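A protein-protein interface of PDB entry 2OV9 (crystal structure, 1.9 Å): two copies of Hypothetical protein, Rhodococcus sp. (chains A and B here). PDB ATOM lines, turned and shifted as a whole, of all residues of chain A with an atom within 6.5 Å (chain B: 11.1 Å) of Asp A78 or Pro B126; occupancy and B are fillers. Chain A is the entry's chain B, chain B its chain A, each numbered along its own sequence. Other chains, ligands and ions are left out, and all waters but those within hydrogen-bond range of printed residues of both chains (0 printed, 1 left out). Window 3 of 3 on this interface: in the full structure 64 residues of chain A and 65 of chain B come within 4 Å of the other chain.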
ATOM      1  N   LEU A  76      22.146  30.167  15.107  1.00  0.00           N
ATOM      2  CA  LEU A  76      20.835  29.568  15.289  1.00  0.00           C
ATOM      3  C   LEU A  76      20.402  29.900  16.701  1.00  0.00           C
ATOM      4  O   LEU A  76      21.152  29.676  17.651  1.00  0.00           O
ATOM      5  CB  LEU A  76      20.898  28.046  15.098  1.00  0.00           C
ATOM      6  CG  LEU A  76      21.330  27.497  13.733  1.00  0.00           C
ATOM      7  CD1 LEU A  76      21.606  26.000  13.814  1.00  0.00           C
ATOM      8  CD2 LEU A  76      20.296  27.814  12.638  1.00  0.00           C
ATOM      9  N   ILE A  77      19.203  30.457  16.828  1.00  0.00           N
ATOM     10  CA  ILE A  77      18.625  30.763  18.124  1.00  0.00           C
ATOM     11  C   ILE A  77      18.084  29.462  18.714  1.00  0.00           C
ATOM     12  O   ILE A  77      17.164  28.863  18.149  1.00  0.00           O
ATOM     13  CB  ILE A  77      17.449  31.785  18.005  1.00  0.00           C
ATOM     14  CG1 ILE A  77      17.784  32.954  17.053  1.00  0.00           C
ATOM     15  CG2 ILE A  77      17.010  32.266  19.381  1.00  0.00           C
ATOM     16  CD1 ILE A  77      18.534  34.138  17.675  1.00  0.00           C
ATOM     17  N   ASP A  78      18.663  29.013  19.830  1.00  0.00           N
ATOM     18  CA  ASP A  78      18.058  27.917  20.590  1.00  0.00           C
ATOM     19  C   ASP A  78      17.021  28.496  21.542  1.00  0.00           C
ATOM     20  O   ASP A  78      17.340  28.888  22.674  1.00  0.00           O
ATOM     21  CB  ASP A  78      19.093  27.078  21.358  1.00  0.00           C
ATOM     22  CG  ASP A  78      18.504  25.759  21.900  1.00  0.00           C
ATOM     23  OD1 ASP A  78      17.285  25.514  21.713  1.00  0.00           O
ATOM     24  OD2 ASP A  78      19.264  24.963  22.511  1.00  0.00           O
ATOM     25  N   MET A  79      15.781  28.550  21.055  1.00  0.00           N
ATOM     26  CA  MET A  79      14.623  29.012  21.818  1.00  0.00           C
ATOM     27  C   MET A  79      14.397  28.187  23.076  1.00  0.00           C
ATOM     28  O   MET A  79      14.025  28.720  24.120  1.00  0.00           O
ATOM     29  CB  MET A  79      13.371  28.928  20.938  1.00  0.00           C
ATOM     30  CG  MET A  79      12.118  29.513  21.565  1.00  0.00           C
ATOM     31  SD  MET A  79      10.653  29.617  20.290  1.00  0.00           S
ATOM     32  CE  MET A  79      10.322  27.710  20.016  1.00  0.00           C
ATOM     33  N   TRP A  80      14.611  26.879  22.960  1.00  0.00           N
ATOM     34  CA  TRP A  80      14.375  25.937  24.060  1.00  0.00           C
ATOM     35  C   TRP A  80      15.460  26.044  25.141  1.00  0.00           C
ATOM     36  O   TRP A  80      15.382  25.387  26.183  1.00  0.00           O
ATOM     37  CB  TRP A  80      14.256  24.502  23.513  1.00  0.00           C
ATOM     38  CG  TRP A  80      13.134  24.372  22.542  1.00  0.00           C
ATOM     39  CD1 TRP A  80      11.832  24.094  22.828  1.00  0.00           C
ATOM     40  CD2 TRP A  80      13.197  24.593  21.126  1.00  0.00           C
ATOM     41  NE1 TRP A  80      11.075  24.099  21.674  1.00  0.00           N
ATOM     42  CE2 TRP A  80      11.889  24.410  20.615  1.00  0.00           C
ATOM     43  CE3 TRP A  80      14.230  24.915  20.238  1.00  0.00           C
ATOM     44  CZ2 TRP A  80      11.593  24.528  19.253  1.00  0.00           C
ATOM     45  CZ3 TRP A  80      13.927  25.042  18.880  1.00  0.00           C
ATOM     46  CH2 TRP A  80      12.620  24.848  18.404  1.00  0.00           C
ATOM     47  N   ASN A  81      16.460  26.883  24.872  1.00  0.00           N
ATOM     48  CA  ASN A  81      17.544  27.165  25.822  1.00  0.00           C
ATOM     49  C   ASN A  81      17.517  28.621  26.304  1.00  0.00           C
ATOM     50  O   ASN A  81      18.469  29.094  26.917  1.00  0.00           O
ATOM     51  CB  ASN A  81      18.901  26.831  25.197  1.00  0.00           C
ATOM     52  CG  ASN A  81      20.016  26.803  26.218  1.00  0.00           C
ATOM     53  OD1 ASN A  81      21.071  27.411  26.018  1.00  0.00           O
ATOM     54  ND2 ASN A  81      19.782  26.119  27.333  1.00  0.00           N
ATOM     55  N   GLY A  82      16.423  29.325  26.008  1.00  0.00           N
ATOM     56  CA  GLY A  82      16.224  30.688  26.490  1.00  0.00           C
ATOM     57  C   GLY A  82      16.851  31.793  25.655  1.00  0.00           C
ATOM     58  O   GLY A  82      16.987  32.932  26.127  1.00  0.00           O
ATOM     59  N   GLU A  83      17.211  31.468  24.414  1.00  0.00           N
ATOM     60  CA  GLU A  83      17.928  32.394  23.529  1.00  0.00           C
ATOM     61  C   GLU A  83      17.018  33.314  22.706  1.00  0.00           C
ATOM     62  O   GLU A  83      17.508  34.198  21.997  1.00  0.00           O
ATOM     63  CB  GLU A  83      18.876  31.624  22.608  1.00  0.00           C
ATOM     64  CG  GLU A  83      19.932  30.842  23.362  1.00  0.00           C
ATOM     65  CD  GLU A  83      20.911  30.099  22.460  1.00  0.00           C
ATOM     66  OE1 GLU A  83      20.784  30.170  21.217  1.00  0.00           O
ATOM     67  OE2 GLU A  83      21.815  29.430  23.008  1.00  0.00           O
ATOM     68  N   GLY A  84      15.705  33.114  22.818  1.00  0.00           N
ATOM     69  CA  GLY A  84      14.735  33.937  22.107  1.00  0.00           C
ATOM     70  C   GLY A  84      14.042  33.089  21.068  1.00  0.00           C
ATOM     71  O   GLY A  84      14.324  31.896  20.946  1.00  0.00           O
ATOM     72  N   THR A  86      13.166  31.283  17.688  1.00  0.00           N
ATOM     73  CA  THR A  86      13.901  30.739  16.526  1.00  0.00           C
ATOM     74  C   THR A  86      13.488  31.410  15.222  1.00  0.00           C
ATOM     75  O   THR A  86      12.380  31.954  15.121  1.00  0.00           O
ATOM     76  CB  THR A  86      13.636  29.239  16.333  1.00  0.00           C
ATOM     77  OG1 THR A  86      12.233  29.041  16.123  1.00  0.00           O
ATOM     78  CG2 THR A  86      14.073  28.444  17.555  1.00  0.00           C
ATOM     79  N   HIS A  88      14.576  29.701  12.005  1.00  0.00           N
ATOM     80  CA  HIS A  88      14.988  28.727  10.993  1.00  0.00           C
ATOM     81  C   HIS A  88      14.071  27.518  10.997  1.00  0.00           C
ATOM     82  O   HIS A  88      14.306  26.540  10.272  1.00  0.00           O
ATOM     83  CB  HIS A  88      16.375  28.215  11.350  1.00  0.00           C
ATOM     84  CG  HIS A  88      16.418  27.503  12.668  1.00  0.00           C
ATOM     85  ND1 HIS A  88      16.734  28.144  13.847  1.00  0.00           N
ATOM     86  CD2 HIS A  88      16.160  26.211  12.998  1.00  0.00           C
ATOM     87  CE1 HIS A  88      16.681  27.278  14.845  1.00  0.00           C
ATOM     88  NE2 HIS A  88      16.337  26.098  14.358  1.00  0.00           N
ATOM     89  N   ARG B  43      20.759  27.175   3.678  1.00  0.00           N
ATOM     90  CA  ARG B  43      22.224  27.173   3.797  1.00  0.00           C
ATOM     91  C   ARG B  43      22.900  28.258   2.951  1.00  0.00           C
ATOM     92  O   ARG B  43      24.102  28.504   3.076  1.00  0.00           O
ATOM     93  CB  ARG B  43      22.777  25.819   3.335  1.00  0.00           C
ATOM     94  CG  ARG B  43      22.365  24.634   4.167  1.00  0.00           C
ATOM     95  CD  ARG B  43      23.236  23.441   3.827  1.00  0.00           C
ATOM     96  NE  ARG B  43      23.446  22.580   4.992  1.00  0.00           N
ATOM     97  CZ  ARG B  43      22.715  21.502   5.263  1.00  0.00           C
ATOM     98  NH1 ARG B  43      21.735  21.148   4.437  1.00  0.00           N
ATOM     99  NH2 ARG B  43      22.960  20.780   6.349  1.00  0.00           N
ATOM    100  N   LEU B 118      16.856  12.734   8.609  1.00  0.00           N
ATOM    101  CA  LEU B 118      16.243  14.056   8.538  1.00  0.00           C
ATOM    102  C   LEU B 118      17.282  15.161   8.339  1.00  0.00           C
ATOM    103  O   LEU B 118      18.432  15.050   8.767  1.00  0.00           O
ATOM    104  CB  LEU B 118      15.364  14.296   9.771  1.00  0.00           C
ATOM    105  CG  LEU B 118      14.069  13.458   9.765  1.00  0.00           C
ATOM    106  CD1 LEU B 118      13.303  13.625  11.071  1.00  0.00           C
ATOM    107  CD2 LEU B 118      13.168  13.822   8.575  1.00  0.00           C
ATOM    108  N   THR B 119      16.845  16.223   7.677  1.00  0.00           N
ATOM    109  CA  THR B 119      17.711  17.254   7.144  1.00  0.00           C
ATOM    110  C   THR B 119      17.365  18.604   7.778  1.00  0.00           C
ATOM    111  O   THR B 119      16.445  18.685   8.600  1.00  0.00           O
ATOM    112  CB  THR B 119      17.537  17.324   5.623  1.00  0.00           C
ATOM    113  OG1 THR B 119      16.145  17.261   5.308  1.00  0.00           O
ATOM    114  CG2 THR B 119      18.247  16.160   4.937  1.00  0.00           C
ATOM    115  N   ILE B 120      18.083  19.665   7.395  1.00  0.00           N
ATOM    116  CA  ILE B 120      17.961  20.953   8.102  1.00  0.00           C
ATOM    117  C   ILE B 120      16.611  21.663   8.047  1.00  0.00           C
ATOM    118  O   ILE B 120      16.345  22.501   8.915  1.00  0.00           O
ATOM    119  CB  ILE B 120      19.038  21.996   7.719  1.00  0.00           C
ATOM    120  CG1 ILE B 120      19.100  22.180   6.194  1.00  0.00           C
ATOM    121  CG2 ILE B 120      20.364  21.678   8.403  1.00  0.00           C
ATOM    122  CD1 ILE B 120      19.594  23.519   5.766  1.00  0.00           C
ATOM    123  N   PRO B 121      15.790  21.419   7.004  1.00  0.00           N
ATOM    124  CA  PRO B 121      14.473  22.046   7.143  1.00  0.00           C
ATOM    125  C   PRO B 121      13.645  21.572   8.343  1.00  0.00           C
ATOM    126  O   PRO B 121      12.726  22.274   8.757  1.00  0.00           O
ATOM    127  CB  PRO B 121      13.779  21.708   5.812  1.00  0.00           C
ATOM    128  CG  PRO B 121      14.913  21.478   4.848  1.00  0.00           C
ATOM    129  CD  PRO B 121      15.934  20.757   5.691  1.00  0.00           C
ATOM    130  N   TYR B 122      13.988  20.415   8.905  1.00  0.00           N
ATOM    131  CA  TYR B 122      13.240  19.822  10.034  1.00  0.00           C
ATOM    132  C   TYR B 122      13.819  20.171  11.403  1.00  0.00           C
ATOM    133  O   TYR B 122      13.332  19.678  12.428  1.00  0.00           O
ATOM    134  CB  TYR B 122      13.099  18.289   9.862  1.00  0.00           C
ATOM    135  CG  TYR B 122      12.496  17.919   8.530  1.00  0.00           C
ATOM    136  CD1 TYR B 122      11.115  17.883   8.354  1.00  0.00           C
ATOM    137  CD2 TYR B 122      13.320  17.692   7.414  1.00  0.00           C
ATOM    138  CE1 TYR B 122      10.559  17.582   7.087  1.00  0.00           C
ATOM    139  CE2 TYR B 122      12.778  17.382   6.157  1.00  0.00           C
ATOM    140  CZ  TYR B 122      11.400  17.339   6.003  1.00  0.00           C
ATOM    141  OH  TYR B 122      10.874  17.040   4.761  1.00  0.00           O
ATOM    142  N   GLN B 123      14.830  21.040  11.413  1.00  0.00           N
ATOM    143  CA  GLN B 123      15.558  21.408  12.619  1.00  0.00           C
ATOM    144  C   GLN B 123      14.720  22.209  13.629  1.00  0.00           C
ATOM    145  O   GLN B 123      13.942  23.085  13.256  1.00  0.00           O
ATOM    146  CB  GLN B 123      16.821  22.179  12.224  1.00  0.00           C
ATOM    147  CG  GLN B 123      17.743  22.585  13.368  1.00  0.00           C
ATOM    148  CD  GLN B 123      18.990  23.259  12.869  1.00  0.00           C
ATOM    149  OE1 GLN B 123      18.935  24.175  12.030  1.00  0.00           O
ATOM    150  NE2 GLN B 123      20.132  22.800  13.355  1.00  0.00           N
ATOM    151  N   GLY B 124      14.847  21.842  14.900  1.00  0.00           N
ATOM    152  CA  GLY B 124      14.341  22.662  15.995  1.00  0.00           C
ATOM    153  C   GLY B 124      15.559  23.085  16.803  1.00  0.00           C
ATOM    154  O   GLY B 124      16.291  23.991  16.413  1.00  0.00           O
ATOM    155  N   PRO B 125      15.813  22.407  17.930  1.00  0.00           N
ATOM    156  CA  PRO B 125      17.076  22.706  18.581  1.00  0.00           C
ATOM    157  C   PRO B 125      18.213  22.429  17.590  1.00  0.00           C
ATOM    158  O   PRO B 125      18.100  21.490  16.785  1.00  0.00           O
ATOM    159  CB  PRO B 125      17.115  21.705  19.750  1.00  0.00           C
ATOM    160  CG  PRO B 125      15.669  21.395  20.013  1.00  0.00           C
ATOM    161  CD  PRO B 125      15.052  21.366  18.637  1.00  0.00           C
ATOM    162  N   PRO B 126      19.305  23.231  17.644  1.00  0.00           N
ATOM    163  CA  PRO B 126      20.449  23.070  16.742  1.00  0.00           C
ATOM    164  C   PRO B 126      20.926  21.620  16.609  1.00  0.00           C
ATOM    165  O   PRO B 126      21.117  20.933  17.618  1.00  0.00           O
ATOM    166  CB  PRO B 126      21.518  23.953  17.382  1.00  0.00           C
ATOM    167  CG  PRO B 126      20.703  25.079  17.995  1.00  0.00           C
ATOM    168  CD  PRO B 126      19.486  24.373  18.562  1.00  0.00           C
ATOM    169  N   GLY B 127      21.092  21.163  15.365  1.00  0.00           N
ATOM    170  CA  GLY B 127      21.500  19.784  15.056  1.00  0.00           C
ATOM    171  C   GLY B 127      20.450  18.710  15.296  1.00  0.00           C
ATOM    172  O   GLY B 127      20.709  17.522  15.083  1.00  0.00           O
ATOM    173  N   HIS B 128      19.253  19.122  15.712  1.00  0.00           N
ATOM    174  CA  HIS B 128      18.232  18.183  16.147  1.00  0.00           C
ATOM    175  C   HIS B 128      16.878  18.427  15.525  1.00  0.00           C
ATOM    176  O   HIS B 128      16.589  19.520  15.002  1.00  0.00           O
ATOM    177  CB  HIS B 128      18.141  18.144  17.676  1.00  0.00           C
ATOM    178  CG  HIS B 128      19.375  17.594  18.323  1.00  0.00           C
ATOM    179  ND1 HIS B 128      20.469  18.377  18.613  1.00  0.00           N
ATOM    180  CD2 HIS B 128      19.702  16.333  18.697  1.00  0.00           C
ATOM    181  CE1 HIS B 128      21.416  17.623  19.152  1.00  0.00           C
ATOM    182  NE2 HIS B 128      20.977  16.378  19.210  1.00  0.00           N
ATOM    183  N   VAL B 129      16.067  17.376  15.538  1.00  0.00           N
ATOM    184  CA  VAL B 129      14.763  17.389  14.903  1.00  0.00           C
ATOM    185  C   VAL B 129      13.789  18.160  15.786  1.00  0.00           C
ATOM    186  O   VAL B 129      13.749  17.931  16.996  1.00  0.00           O
ATOM    187  CB  VAL B 129      14.240  15.946  14.715  1.00  0.00           C
ATOM    188  CG1 VAL B 129      12.778  15.959  14.235  1.00  0.00           C
ATOM    189  CG2 VAL B 129      15.145  15.148  13.753  1.00  0.00           C
ATOM    190  N   HIS B 130      13.015  19.076  15.186  1.00  0.00           N
ATOM    191  CA  HIS B 130      11.975  19.797  15.923  1.00  0.00           C
ATOM    192  C   HIS B 130      11.017  18.786  16.576  1.00  0.00           C
ATOM    193  O   HIS B 130      10.521  17.870  15.910  1.00  0.00           O
ATOM    194  CB  HIS B 130      11.209  20.678  14.949  1.00  0.00           C
ATOM    195  CG  HIS B 130      10.418  21.778  15.593  1.00  0.00           C
ATOM    196  ND1 HIS B 130       9.360  21.539  16.440  1.00  0.00           N
ATOM    197  CD2 HIS B 130      10.496  23.123  15.462  1.00  0.00           C
ATOM    198  CE1 HIS B 130       8.838  22.690  16.833  1.00  0.00           C
ATOM    199  NE2 HIS B 130       9.519  23.667  16.262  1.00  0.00           N
ATOM    200  N   GLY B 131      10.739  18.965  17.864  1.00  0.00           N
ATOM    201  CA  GLY B 131       9.806  18.091  18.575  1.00  0.00           C
ATOM    202  C   GLY B 131       8.473  17.964  17.858  1.00  0.00           C
ATOM    203  O   GLY B 131       7.829  16.911  17.920  1.00  0.00           O
ATOM    204  N   PRO B 165      17.138  13.485  22.939  1.00  0.00           N
ATOM    205  CA  PRO B 165      17.118  14.355  21.736  1.00  0.00           C
ATOM    206  C   PRO B 165      17.126  13.535  20.442  1.00  0.00           C
ATOM    207  O   PRO B 165      17.716  12.453  20.382  1.00  0.00           O
ATOM    208  CB  PRO B 165      18.420  15.150  21.847  1.00  0.00           C
ATOM    209  CG  PRO B 165      18.834  15.033  23.296  1.00  0.00           C
ATOM    210  CD  PRO B 165      18.348  13.698  23.749  1.00  0.00           C
ATOM    211  N   THR B 166      16.439  14.032  19.425  1.00  0.00           N
ATOM    212  CA  THR B 166      16.380  13.339  18.144  1.00  0.00           C
ATOM    213  C   THR B 166      17.289  14.043  17.134  1.00  0.00           C
ATOM    214  O   THR B 166      17.001  15.159  16.722  1.00  0.00           O
ATOM    215  CB  THR B 166      14.938  13.326  17.592  1.00  0.00           C
ATOM    216  OG1 THR B 166      14.033  13.036  18.664  1.00  0.00           O
ATOM    217  CG2 THR B 166      14.801  12.259  16.527  1.00  0.00           C
ATOM    218  N   PRO B 167      18.388  13.384  16.725  1.00  0.00           N
ATOM    219  CA  PRO B 167      19.372  14.059  15.883  1.00  0.00           C
ATOM    220  C   PRO B 167      19.008  14.139  14.409  1.00  0.00           C
ATOM    221  O   PRO B 167      18.392  13.222  13.862  1.00  0.00           O
ATOM    222  CB  PRO B 167      20.646  13.205  16.071  1.00  0.00           C
ATOM    223  CG  PRO B 167      20.132  11.846  16.381  1.00  0.00           C
ATOM    224  CD  PRO B 167      18.793  12.001  17.063  1.00  0.00           C
ATOM    225  N   LEU B 168      19.390  15.245  13.779  1.00  0.00           N
ATOM    226  CA  LEU B 168      19.398  15.346  12.325  1.00  0.00           C
ATOM    227  C   LEU B 168      20.567  14.539  11.775  1.00  0.00           C
ATOM    228  O   LEU B 168      21.441  14.124  12.526  1.00  0.00           O
ATOM    229  CB  LEU B 168      19.562  16.793  11.893  1.00  0.00           C
ATOM    230  CG  LEU B 168      18.474  17.771  12.322  1.00  0.00           C
ATOM    231  CD1 LEU B 168      18.942  19.192  12.056  1.00  0.00           C
ATOM    232  CD2 LEU B 168      17.171  17.468  11.586  1.00  0.00           C
ATOM    233  N   PHE B 169      20.552  14.330  10.458  1.00  0.00           N
ATOM    234  CA  PHE B 169      21.674  13.779   9.687  1.00  0.00           C
ATOM    235  C   PHE B 169      22.052  12.338  10.009  1.00  0.00           C
ATOM    236  O   PHE B 169      23.144  11.907   9.693  1.00  0.00           O
ATOM    237  CB  PHE B 169      22.913  14.703   9.754  1.00  0.00           C
ATOM    238  CG  PHE B 169      22.583  16.179   9.734  1.00  0.00           C
ATOM    239  CD1 PHE B 169      21.897  16.749   8.656  1.00  0.00           C
ATOM    240  CD2 PHE B 169      22.966  16.998  10.789  1.00  0.00           C
ATOM    241  CE1 PHE B 169      21.592  18.122   8.642  1.00  0.00           C
ATOM    242  CE2 PHE B 169      22.671  18.367  10.782  1.00  0.00           C
ATOM    243  CZ  PHE B 169      21.976  18.926   9.707  1.00  0.00           C
ATOM    244  N   GLU B 170      21.139  11.581  10.614  1.00  0.00           N
ATOM    245  CA  GLU B 170      21.395  10.155  10.839  1.00  0.00           C
ATOM    246  C   GLU B 170      20.136   9.289  10.751  1.00  0.00           C
ATOM    247  O   GLU B 170      19.019   9.796  10.962  1.00  0.00           O
ATOM    248  CB  GLU B 170      22.170   9.924  12.140  1.00  0.00           C
ATOM    249  CG  GLU B 170      21.413  10.256  13.383  1.00  0.00           C
ATOM    250  CD  GLU B 170      22.222   9.965  14.620  1.00  0.00           C
ATOM    251  OE1 GLU B 170      23.103  10.790  14.961  1.00  0.00           O
ATOM    252  OE2 GLU B 170      21.961   8.924  15.257  1.00  0.00           O
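O of Gly B124 sits at hydrogen-bond distance from NE2 of His A88 (2.9 Å).
The backbone carbonyl oxygen (O) of Tyr B122 lies within hydrogen-bond range of the backbone NH (N) of His B130 (2.8 Å). The side-chain carboxylate of Glu A83 is in hydrogen-bond range of the backbone NH of Asp A78, at 2.8 Å. O of Pro B126 is in hydrogen-bond range of ND1 of His B128. The backbone NH (N) of Gly B127 sits close to the side-chain amide nitrogen (NE2) of Gln B123 (2.8 Å). The backbone NH (N) of Trp A80 lies close to the side-chain carboxylate (OD1) of Asp A78 (3.3 Å).
CD1 of Leu A76 touches NE2 of Gln B123 (3.6 Å). Pro B126 touches Asp A78. Gly B124 touches Trp A80. Pro B125 touches Trp A80 (N to CZ3, 3.4 Å). Trp A80 touches His B130. CD2 of His A88 touches OE1 of Gln B123 (3.6 Å).
Of chain B, only Pro B126 (3.7 Å) comes within 4 Å of Asp A78. No residue of chain B comes within 4 Å of Met A79. No residue of chain B comes within 4 Å of Gly A82. No residue of chain B comes within 4 Å of Gly A84. Printed residues of chain A within 4 Å of Gly B124: Trp A80 and His A88. Printed residues of chain A within 4 Å of Pro B126: Asp A78. Printed residues of chain A within 4 Å of His B130: Trp A80. Leu B168 touches none of the printed residues of chain A. The nearest residue of chain B that does not touch Asp A78 is Pro B125 (4.2 Å). The nearest printed residue of chain A that does not touch Pro B125 is Asp A78 (4.2 Å).
Hydrophobic or aromatic side chains of chain B within 4 Å of the printed part of chain A: Pro B125, Pro B126 and His B130. Of the 11 printed residues of chain A, 4 touch a printed residue of chain B. Printed residues of chain A that touch a printed residue of chain B: Leu A76, Asp A78, Trp A80 and His A88. Hydrophobic or aromatic side chains of chain A that line the printed part of chain B: Leu A76, Trp A80 and His A88. Among the printed residues, 7 pairs touch across the chains. Among the printed residues, no Asp or Glu carboxylate lies within 4 Å of a Lys or Arg side-chain nitrogen of the other chain.
No position is printed for both chains.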
